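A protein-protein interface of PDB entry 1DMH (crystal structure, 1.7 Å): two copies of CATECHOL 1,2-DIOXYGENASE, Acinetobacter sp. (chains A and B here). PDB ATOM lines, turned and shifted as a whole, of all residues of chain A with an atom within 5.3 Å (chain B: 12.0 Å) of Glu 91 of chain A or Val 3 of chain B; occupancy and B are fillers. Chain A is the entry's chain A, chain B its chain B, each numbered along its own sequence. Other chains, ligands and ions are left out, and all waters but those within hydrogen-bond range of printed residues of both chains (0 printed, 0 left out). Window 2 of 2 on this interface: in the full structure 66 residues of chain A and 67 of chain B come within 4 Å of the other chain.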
ATOM      1  N   MET A  86     -12.355  24.404   7.846  1.00  0.00           N
ATOM      2  CA  MET A  86     -12.643  25.793   7.486  1.00  0.00           C
ATOM      3  C   MET A  86     -14.149  26.013   7.522  1.00  0.00           C
ATOM      4  O   MET A  86     -14.625  27.072   7.953  1.00  0.00           O
ATOM      5  CB  MET A  86     -12.097  26.128   6.090  1.00  0.00           C
ATOM      6  CG  MET A  86     -10.584  26.110   6.016  1.00  0.00           C
ATOM      7  SD  MET A  86      -9.979  26.398   4.329  1.00  0.00           S
ATOM      8  CE  MET A  86     -10.353  28.205   4.163  1.00  0.00           C
ATOM      9  N   ARG A  87     -14.906  25.016   7.069  1.00  0.00           N
ATOM     10  CA  ARG A  87     -16.351  25.135   7.074  1.00  0.00           C
ATOM     11  C   ARG A  87     -16.829  25.214   8.519  1.00  0.00           C
ATOM     12  O   ARG A  87     -17.681  26.058   8.856  1.00  0.00           O
ATOM     13  CB  ARG A  87     -16.980  23.951   6.361  1.00  0.00           C
ATOM     14  CG  ARG A  87     -16.684  23.905   4.875  1.00  0.00           C
ATOM     15  CD  ARG A  87     -17.266  22.636   4.297  1.00  0.00           C
ATOM     16  NE  ARG A  87     -18.724  22.694   4.229  1.00  0.00           N
ATOM     17  CZ  ARG A  87     -19.546  21.694   4.561  1.00  0.00           C
ATOM     18  NH1 ARG A  87     -19.077  20.517   5.008  1.00  0.00           N
ATOM     19  NH2 ARG A  87     -20.855  21.864   4.406  1.00  0.00           N
ATOM     20  N   MET A  88     -16.285  24.351   9.381  1.00  0.00           N
ATOM     21  CA  MET A  88     -16.668  24.376  10.790  1.00  0.00           C
ATOM     22  C   MET A  88     -16.353  25.727  11.437  1.00  0.00           C
ATOM     23  O   MET A  88     -17.166  26.252  12.223  1.00  0.00           O
ATOM     24  CB  MET A  88     -15.995  23.248  11.542  1.00  0.00           C
ATOM     25  CG  MET A  88     -16.637  21.930  11.237  1.00  0.00           C
ATOM     26  SD  MET A  88     -15.975  20.582  12.247  1.00  0.00           S
ATOM     27  CE  MET A  88     -14.658  19.901  11.237  1.00  0.00           C
ATOM     28  N   ASP A  89     -15.194  26.299  11.109  1.00  0.00           N
ATOM     29  CA  ASP A  89     -14.837  27.613  11.647  1.00  0.00           C
ATOM     30  C   ASP A  89     -15.809  28.692  11.180  1.00  0.00           C
ATOM     31  O   ASP A  89     -16.237  29.547  11.967  1.00  0.00           O
ATOM     32  CB  ASP A  89     -13.441  28.032  11.242  1.00  0.00           C
ATOM     33  CG  ASP A  89     -12.374  27.256  11.959  1.00  0.00           C
ATOM     34  OD1 ASP A  89     -12.651  26.685  13.030  1.00  0.00           O
ATOM     35  OD2 ASP A  89     -11.247  27.238  11.455  1.00  0.00           O
ATOM     36  N   ALA A  90     -16.150  28.650   9.896  1.00  0.00           N
ATOM     37  CA  ALA A  90     -17.084  29.614   9.333  1.00  0.00           C
ATOM     38  C   ALA A  90     -18.427  29.514  10.062  1.00  0.00           C
ATOM     39  O   ALA A  90     -19.026  30.531  10.423  1.00  0.00           O
ATOM     40  CB  ALA A  90     -17.276  29.340   7.831  1.00  0.00           C
ATOM     41  N   GLU A  91     -18.898  28.288  10.269  1.00  0.00           N
ATOM     42  CA  GLU A  91     -20.171  28.061  10.936  1.00  0.00           C
ATOM     43  C   GLU A  91     -20.130  28.581  12.372  1.00  0.00           C
ATOM     44  O   GLU A  91     -21.083  29.201  12.833  1.00  0.00           O
ATOM     45  CB  GLU A  91     -20.492  26.586  10.919  1.00  0.00           C
ATOM     46  CG  GLU A  91     -21.890  26.279  11.296  1.00  0.00           C
ATOM     47  CD  GLU A  91     -22.115  24.787  11.431  1.00  0.00           C
ATOM     48  OE1 GLU A  91     -21.579  24.182  12.396  1.00  0.00           O
ATOM     49  OE2 GLU A  91     -22.811  24.210  10.564  1.00  0.00           O
ATOM     50  N   ASP A  92     -19.027  28.343  13.077  1.00  0.00           N
ATOM     51  CA  ASP A  92     -18.893  28.853  14.442  1.00  0.00           C
ATOM     52  C   ASP A  92     -18.865  30.391  14.444  1.00  0.00           C
ATOM     53  O   ASP A  92     -19.479  31.026  15.311  1.00  0.00           O
ATOM     54  CB  ASP A  92     -17.612  28.356  15.124  1.00  0.00           C
ATOM     55  CG  ASP A  92     -17.683  26.900  15.554  1.00  0.00           C
ATOM     56  OD1 ASP A  92     -18.753  26.265  15.472  1.00  0.00           O
ATOM     57  OD2 ASP A  92     -16.633  26.396  16.010  1.00  0.00           O
ATOM     58  N   ALA A  93     -18.141  30.978  13.492  1.00  0.00           N
ATOM     59  CA  ALA A  93     -18.031  32.428  13.390  1.00  0.00           C
ATOM     60  C   ALA A  93     -19.418  33.025  13.211  1.00  0.00           C
ATOM     61  O   ALA A  93     -19.748  34.057  13.805  1.00  0.00           O
ATOM     62  CB  ALA A  93     -17.139  32.815  12.217  1.00  0.00           C
ATOM     63  N   ALA A  94     -20.242  32.374  12.401  1.00  0.00           N
ATOM     64  CA  ALA A  94     -21.595  32.869  12.172  1.00  0.00           C
ATOM     65  C   ALA A  94     -22.449  32.780  13.450  1.00  0.00           C
ATOM     66  O   ALA A  94     -23.362  33.583  13.641  1.00  0.00           O
ATOM     67  CB  ALA A  94     -22.260  32.093  11.024  1.00  0.00           C
ATOM     68  N   LEU A  95     -22.155  31.815  14.319  1.00  0.00           N
ATOM     69  CA  LEU A  95     -22.901  31.643  15.568  1.00  0.00           C
ATOM     70  C   LEU A  95     -22.312  32.465  16.698  1.00  0.00           C
ATOM     71  O   LEU A  95     -22.746  32.352  17.838  1.00  0.00           O
ATOM     72  CB  LEU A  95     -22.907  30.175  16.002  1.00  0.00           C
ATOM     73  CG  LEU A  95     -23.663  29.204  15.101  1.00  0.00           C
ATOM     74  CD1 LEU A  95     -23.502  27.760  15.600  1.00  0.00           C
ATOM     75  CD2 LEU A  95     -25.125  29.624  15.078  1.00  0.00           C
ATOM     76  N   ASN A 301     -22.628  20.529  17.893  1.00  0.00           N
ATOM     77  CA  ASN A 301     -22.877  20.660  16.464  1.00  0.00           C
ATOM     78  C   ASN A 301     -21.696  20.334  15.549  1.00  0.00           C
ATOM     79  O   ASN A 301     -21.844  20.331  14.324  1.00  0.00           O
ATOM     80  CB  ASN A 301     -23.381  22.071  16.139  1.00  0.00           C
ATOM     81  CG  ASN A 301     -22.391  23.162  16.516  1.00  0.00           C
ATOM     82  OD1 ASN A 301     -22.424  24.262  15.944  1.00  0.00           O
ATOM     83  ND2 ASN A 301     -21.530  22.886  17.489  1.00  0.00           N
ATOM     84  N   VAL B   3     -23.967  29.807   5.450  1.00  0.00           N
ATOM     85  CA  VAL B   3     -22.467  29.653   5.498  1.00  0.00           C
ATOM     86  C   VAL B   3     -21.894  29.094   4.181  1.00  0.00           C
ATOM     87  O   VAL B   3     -22.059  27.921   3.866  1.00  0.00           O
ATOM     88  CB  VAL B   3     -22.037  28.726   6.674  1.00  0.00           C
ATOM     89  CG1 VAL B   3     -20.519  28.481   6.635  1.00  0.00           C
ATOM     90  CG2 VAL B   3     -22.443  29.359   8.013  1.00  0.00           C
ATOM     91  N   LYS B   4     -21.213  29.946   3.423  1.00  0.00           N
ATOM     92  CA  LYS B   4     -20.645  29.552   2.140  1.00  0.00           C
ATOM     93  C   LYS B   4     -19.240  30.111   2.003  1.00  0.00           C
ATOM     94  O   LYS B   4     -19.053  31.325   2.079  1.00  0.00           O
ATOM     95  CB  LYS B   4     -21.500  30.105   1.012  1.00  0.00           C
ATOM     96  CG  LYS B   4     -22.969  29.679   1.057  1.00  0.00           C
ATOM     97  CD  LYS B   4     -23.128  28.195   0.799  1.00  0.00           C
ATOM     98  CE  LYS B   4     -24.586  27.842   0.543  1.00  0.00           C
ATOM     99  NZ  LYS B   4     -24.734  26.427   0.112  1.00  0.00           N
ATOM    100  N   ILE B   5     -18.252  29.255   1.774  1.00  0.00           N
ATOM    101  CA  ILE B   5     -16.887  29.755   1.656  1.00  0.00           C
ATOM    102  C   ILE B   5     -16.152  29.366   0.363  1.00  0.00           C
ATOM    103  O   ILE B   5     -15.068  29.880   0.082  1.00  0.00           O
ATOM    104  CB  ILE B   5     -16.029  29.285   2.866  1.00  0.00           C
ATOM    105  CG1 ILE B   5     -15.933  27.754   2.896  1.00  0.00           C
ATOM    106  CG2 ILE B   5     -16.663  29.764   4.173  1.00  0.00           C
ATOM    107  CD1 ILE B   5     -14.962  27.241   3.954  1.00  0.00           C
ATOM    108  N   PHE B   6     -16.739  28.477  -0.433  1.00  0.00           N
ATOM    109  CA  PHE B   6     -16.058  28.040  -1.646  1.00  0.00           C
ATOM    110  C   PHE B   6     -15.525  29.168  -2.549  1.00  0.00           C
ATOM    111  O   PHE B   6     -14.378  29.138  -2.987  1.00  0.00           O
ATOM    112  CB  PHE B   6     -16.960  27.120  -2.471  1.00  0.00           C
ATOM    113  CG  PHE B   6     -16.329  26.666  -3.777  1.00  0.00           C
ATOM    114  CD1 PHE B   6     -15.382  25.643  -3.797  1.00  0.00           C
ATOM    115  CD2 PHE B   6     -16.623  27.323  -4.976  1.00  0.00           C
ATOM    116  CE1 PHE B   6     -14.734  25.280  -4.982  1.00  0.00           C
ATOM    117  CE2 PHE B   6     -15.974  26.962  -6.169  1.00  0.00           C
ATOM    118  CZ  PHE B   6     -15.027  25.936  -6.165  1.00  0.00           C
ATOM    119  N   ASN B   7     -16.348  30.168  -2.838  1.00  0.00           N
ATOM    120  CA  ASN B   7     -15.888  31.229  -3.722  1.00  0.00           C
ATOM    121  C   ASN B   7     -15.176  32.399  -3.072  1.00  0.00           C
ATOM    122  O   ASN B   7     -15.196  33.503  -3.596  1.00  0.00           O
ATOM    123  CB  ASN B   7     -17.034  31.706  -4.641  1.00  0.00           C
ATOM    124  CG  ASN B   7     -17.177  30.823  -5.927  1.00  0.00           C
ATOM    125  OD1 ASN B   7     -18.215  30.166  -6.155  1.00  0.00           O
ATOM    126  ND2 ASN B   7     -16.122  30.810  -6.761  1.00  0.00           N
ATOM    127  N   THR B   8     -14.536  32.157  -1.935  1.00  0.00           N
ATOM    128  CA  THR B   8     -13.752  33.194  -1.260  1.00  0.00           C
ATOM    129  C   THR B   8     -12.298  33.011  -1.708  1.00  0.00           C
ATOM    130  O   THR B   8     -11.900  31.910  -2.096  1.00  0.00           O
ATOM    131  CB  THR B   8     -13.804  33.060   0.275  1.00  0.00           C
ATOM    132  OG1 THR B   8     -13.285  31.782   0.679  1.00  0.00           O
ATOM    133  CG2 THR B   8     -15.245  33.218   0.768  1.00  0.00           C
ATOM    134  N   VAL B  11     -10.245  30.057  -0.060  1.00  0.00           N
ATOM    135  CA  VAL B  11     -10.444  28.721  -0.585  1.00  0.00           C
ATOM    136  C   VAL B  11      -9.892  28.579  -2.000  1.00  0.00           C
ATOM    137  O   VAL B  11      -9.252  27.572  -2.310  1.00  0.00           O
ATOM    138  CB  VAL B  11     -11.923  28.342  -0.545  1.00  0.00           C
ATOM    139  CG1 VAL B  11     -12.153  27.013  -1.273  1.00  0.00           C
ATOM    140  CG2 VAL B  11     -12.378  28.243   0.923  1.00  0.00           C
ATOM    141  N   TYR B  42     -14.954  20.186  -3.885  1.00  0.00           N
ATOM    142  CA  TYR B  42     -15.084  21.152  -2.783  1.00  0.00           C
ATOM    143  C   TYR B  42     -16.404  21.879  -2.942  1.00  0.00           C
ATOM    144  O   TYR B  42     -17.123  22.077  -1.978  1.00  0.00           O
ATOM    145  CB  TYR B  42     -13.957  22.186  -2.806  1.00  0.00           C
ATOM    146  CG  TYR B  42     -12.678  21.778  -2.124  1.00  0.00           C
ATOM    147  CD1 TYR B  42     -12.152  20.491  -2.259  1.00  0.00           C
ATOM    148  CD2 TYR B  42     -11.914  22.728  -1.455  1.00  0.00           C
ATOM    149  CE1 TYR B  42     -10.879  20.172  -1.752  1.00  0.00           C
ATOM    150  CE2 TYR B  42     -10.654  22.420  -0.951  1.00  0.00           C
ATOM    151  CZ  TYR B  42     -10.145  21.148  -1.107  1.00  0.00           C
ATOM    152  OH  TYR B  42      -8.885  20.904  -0.636  1.00  0.00           O
ATOM    153  N   LYS B  43     -16.725  22.267  -4.172  1.00  0.00           N
ATOM    154  CA  LYS B  43     -17.971  22.973  -4.427  1.00  0.00           C
ATOM    155  C   LYS B  43     -19.185  22.075  -4.169  1.00  0.00           C
ATOM    156  O   LYS B  43     -20.176  22.514  -3.590  1.00  0.00           O
ATOM    157  CB  LYS B  43     -18.006  23.505  -5.864  1.00  0.00           C
ATOM    158  CG  LYS B  43     -19.317  24.242  -6.218  1.00  0.00           C
ATOM    159  CD  LYS B  43     -19.254  24.891  -7.595  1.00  0.00           C
ATOM    160  CE  LYS B  43     -20.670  25.320  -8.064  1.00  0.00           C
ATOM    161  NZ  LYS B  43     -21.449  26.104  -7.042  1.00  0.00           N
ATOM    162  N   ALA B  44     -19.122  20.823  -4.599  1.00  0.00           N
ATOM    163  CA  ALA B  44     -20.244  19.912  -4.376  1.00  0.00           C
ATOM    164  C   ALA B  44     -20.497  19.691  -2.886  1.00  0.00           C
ATOM    165  O   ALA B  44     -21.652  19.563  -2.464  1.00  0.00           O
ATOM    166  CB  ALA B  44     -19.996  18.576  -5.085  1.00  0.00           C
ATOM    167  N   ILE B  45     -19.431  19.641  -2.088  1.00  0.00           N
ATOM    168  CA  ILE B  45     -19.583  19.464  -0.645  1.00  0.00           C
ATOM    169  C   ILE B  45     -20.382  20.647  -0.070  1.00  0.00           C
ATOM    170  O   ILE B  45     -21.234  20.470   0.814  1.00  0.00           O
ATOM    171  CB  ILE B  45     -18.185  19.357   0.061  1.00  0.00           C
ATOM    172  CG1 ILE B  45     -17.585  17.973  -0.260  1.00  0.00           C
ATOM    173  CG2 ILE B  45     -18.318  19.624   1.597  1.00  0.00           C
ATOM    174  CD1 ILE B  45     -16.152  17.750   0.205  1.00  0.00           C
ATOM    175  N   GLU B  46     -20.110  21.848  -0.569  1.00  0.00           N
ATOM    176  CA  GLU B  46     -20.830  23.030  -0.118  1.00  0.00           C
ATOM    177  C   GLU B  46     -22.273  23.082  -0.667  1.00  0.00           C
ATOM    178  O   GLU B  46     -23.232  23.257   0.099  1.00  0.00           O
ATOM    179  CB  GLU B  46     -20.055  24.282  -0.528  1.00  0.00           C
ATOM    180  CG  GLU B  46     -20.724  25.535  -0.091  1.00  0.00           C
ATOM    181  CD  GLU B  46     -19.839  26.739  -0.283  1.00  0.00           C
ATOM    182  OE1 GLU B  46     -18.865  26.859   0.474  1.00  0.00           O
ATOM    183  OE2 GLU B  46     -20.129  27.545  -1.203  1.00  0.00           O
ATOM    184  N   ASP B  47     -22.427  22.905  -1.979  1.00  0.00           N
ATOM    185  CA  ASP B  47     -23.748  22.934  -2.614  1.00  0.00           C
ATOM    186  C   ASP B  47     -24.732  21.929  -2.054  1.00  0.00           C
ATOM    187  O   ASP B  47     -25.896  22.247  -1.865  1.00  0.00           O
ATOM    188  CB  ASP B  47     -23.635  22.690  -4.119  1.00  0.00           C
ATOM    189  CG  ASP B  47     -23.076  23.887  -4.871  1.00  0.00           C
ATOM    190  OD1 ASP B  47     -22.850  24.948  -4.242  1.00  0.00           O
ATOM    191  OD2 ASP B  47     -22.871  23.760  -6.101  1.00  0.00           O
ATOM    192  N   LEU B  48     -24.276  20.707  -1.805  1.00  0.00           N
ATOM    193  CA  LEU B  48     -25.153  19.663  -1.265  1.00  0.00           C
ATOM    194  C   LEU B  48     -25.121  19.567   0.266  1.00  0.00           C
ATOM    195  O   LEU B  48     -25.792  18.705   0.856  1.00  0.00           O
ATOM    196  CB  LEU B  48     -24.767  18.311  -1.873  1.00  0.00           C
ATOM    197  CG  LEU B  48     -25.061  18.138  -3.371  1.00  0.00           C
ATOM    198  CD1 LEU B  48     -24.326  16.933  -3.921  1.00  0.00           C
ATOM    199  CD2 LEU B  48     -26.551  17.983  -3.570  1.00  0.00           C
ATOM    200  N   ASN B  49     -24.357  20.459   0.895  1.00  0.00           N
ATOM    201  CA  ASN B  49     -24.177  20.497   2.345  1.00  0.00           C
ATOM    202  C   ASN B  49     -23.799  19.099   2.884  1.00  0.00           C
ATOM    203  O   ASN B  49     -24.444  18.533   3.792  1.00  0.00           O
ATOM    204  CB  ASN B  49     -25.443  21.010   3.055  1.00  0.00           C
ATOM    205  CG  ASN B  49     -25.182  21.368   4.534  1.00  0.00           C
ATOM    206  OD1 ASN B  49     -26.099  21.330   5.377  1.00  0.00           O
ATOM    207  ND2 ASN B  49     -23.935  21.745   4.850  1.00  0.00           N
ATOM    208  N   ILE B  50     -22.748  18.528   2.311  1.00  0.00           N
ATOM    209  CA  ILE B  50     -22.266  17.218   2.755  1.00  0.00           C
ATOM    210  C   ILE B  50     -21.581  17.422   4.113  1.00  0.00           C
ATOM    211  O   ILE B  50     -20.690  18.259   4.265  1.00  0.00           O
ATOM    212  CB  ILE B  50     -21.291  16.634   1.702  1.00  0.00           C
ATOM    213  CG1 ILE B  50     -22.091  16.301   0.443  1.00  0.00           C
ATOM    214  CG2 ILE B  50     -20.522  15.430   2.262  1.00  0.00           C
ATOM    215  CD1 ILE B  50     -21.233  15.975  -0.756  1.00  0.00           C
ATOM    216  N   THR B  51     -22.010  16.665   5.111  1.00  0.00           N
ATOM    217  CA  THR B  51     -21.455  16.784   6.458  1.00  0.00           C
ATOM    218  C   THR B  51     -20.142  16.001   6.572  1.00  0.00           C
ATOM    219  O   THR B  51     -19.804  15.218   5.673  1.00  0.00           O
ATOM    220  CB  THR B  51     -22.455  16.202   7.474  1.00  0.00           C
ATOM    221  OG1 THR B  51     -22.568  14.787   7.268  1.00  0.00           O
ATOM    222  CG2 THR B  51     -23.849  16.807   7.260  1.00  0.00           C
ATOM    223  N   SER B  52     -19.392  16.198   7.660  1.00  0.00           N
ATOM    224  CA  SER B  52     -18.154  15.421   7.837  1.00  0.00           C
ATOM    225  C   SER B  52     -18.463  13.926   7.965  1.00  0.00           C
ATOM    226  O   SER B  52     -17.724  13.083   7.441  1.00  0.00           O
ATOM    227  CB  SER B  52     -17.372  15.863   9.079  1.00  0.00           C
ATOM    228  OG  SER B  52     -16.828  17.155   8.890  1.00  0.00           O
ATOM    229  N   ASP B  53     -19.544  13.595   8.670  1.00  0.00           N
ATOM    230  CA  ASP B  53     -19.927  12.191   8.832  1.00  0.00           C
ATOM    231  C   ASP B  53     -20.172  11.572   7.460  1.00  0.00           C
ATOM    232  O   ASP B  53     -19.733  10.453   7.199  1.00  0.00           O
ATOM    233  CB  ASP B  53     -21.190  12.054   9.696  1.00  0.00           C
ATOM    234  CG  ASP B  53     -20.950  12.457  11.142  1.00  0.00           C
ATOM    235  OD1 ASP B  53     -19.859  13.006  11.440  1.00  0.00           O
ATOM    236  OD2 ASP B  53     -21.863  12.238  11.980  1.00  0.00           O
ATOM    237  N   GLU B  54     -20.871  12.288   6.581  1.00  0.00           N
ATOM    238  CA  GLU B  54     -21.120  11.751   5.249  1.00  0.00           C
ATOM    239  C   GLU B  54     -19.809  11.624   4.501  1.00  0.00           C
ATOM    240  O   GLU B  54     -19.503  10.574   3.912  1.00  0.00           O
ATOM    241  CB  GLU B  54     -22.081  12.652   4.469  1.00  0.00           C
ATOM    242  CG  GLU B  54     -23.522  12.554   4.962  1.00  0.00           C
ATOM    243  CD  GLU B  54     -24.460  13.508   4.246  1.00  0.00           C
ATOM    244  OE1 GLU B  54     -24.061  14.656   3.961  1.00  0.00           O
ATOM    245  OE2 GLU B  54     -25.617  13.128   3.990  1.00  0.00           O
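The guanidinium group of Arg 87 of chain A lies within hydrogen-bond range of the backbone carbonyl oxygen of Ile 50 of chain B (2.9 Å). ND2 of Asn 49 of chain B lies close to NH2 of Arg 87 of chain A.
The backbone NH (N) of Ile 5 of chain B lies within hydrogen-bond range of the side-chain carboxylate (OE1) of Glu 46 of chain B, 2.8 Å away. The side-chain hydroxyl (OG1) of Thr 8 of chain B sits at hydrogen-bond distance from the backbone carbonyl oxygen (O) of Ile 5 of chain B, 2.7 Å away. The backbone NH (N) of Ile 50 of chain B sits at hydrogen-bond distance from the backbone carbonyl oxygen (O) of Ile 45 of chain B (2.9 Å).
Among the printed residues, merely in contact across the chains: Ala 90 of chain A with Val 3 of chain B (3.6 Å), Arg 87 of chain A with Ile 45 of chain B (3.6 Å), Ala 90 of chain A with Ile 5 of chain B (3.7 Å), Met 86 of chain A with Ile 5 of chain B (3.7 Å), Met 86 of chain A with Val 11 of chain B (3.8 Å), Arg 87 of chain A with Ile 5 of chain B (3.8 Å) and Glu 91 of chain A with Val 3 of chain B (3.9 Å).
Of the printed residues of chain B, Met 86 of chain A touches Ile 5 (3.7 Å) and Val 11 (3.8 Å). No residue of chain B comes within 4 Å of Asp 89 of chain A. Ala 90 of chain A touches just these residues of chain B: Val 3 (3.6 Å) and Ile 5 (3.7 Å). Glu 91 of chain A touches one residue of chain B. No residue of chain B comes within 4 Å of Asp 92 of chain A. No residue of chain B comes within 4 Å of Ala 93 of chain A. No residue of chain B comes within 4 Å of Ala 94 of chain A. Of chain A, only Ala 90 (3.6 Å) and Glu 91 (3.9 Å) come within 4 Å of Val 3 of chain B. Printed residues of chain A within 4 Å of Ile 5 of chain B: Met 86 (3.7 Å), Arg 87 (3.8 Å) and Ala 90 (3.7 Å). Printed residues of chain A within 4 Å of Val 11 of chain B: Met 86 (3.8 Å). Tyr 42 of chain B touches none of the printed residues of chain A. Printed residues of chain A within 4 Å of Ile 45 of chain B: Arg 87.
Of the 11 printed residues of chain A, 4 touch a printed residue of chain B. Hydrophobic or aromatic side chains of chain A that line the printed part of chain B: Met 86 and Ala 90. Of the 20 printed residues of chain B, 6 touch a printed residue of chain A. Hydrophobic or aromatic side chains of chain B that line the printed part of chain A: Val 3, Ile 5, Val 11 and Ile 45. Among the printed residues, 9 pairs touch across the chains.
No position is printed for both chains. Of the 9 pairs that touch across the chains among the printed residues, none has its exchanged pair printed and touching as well.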
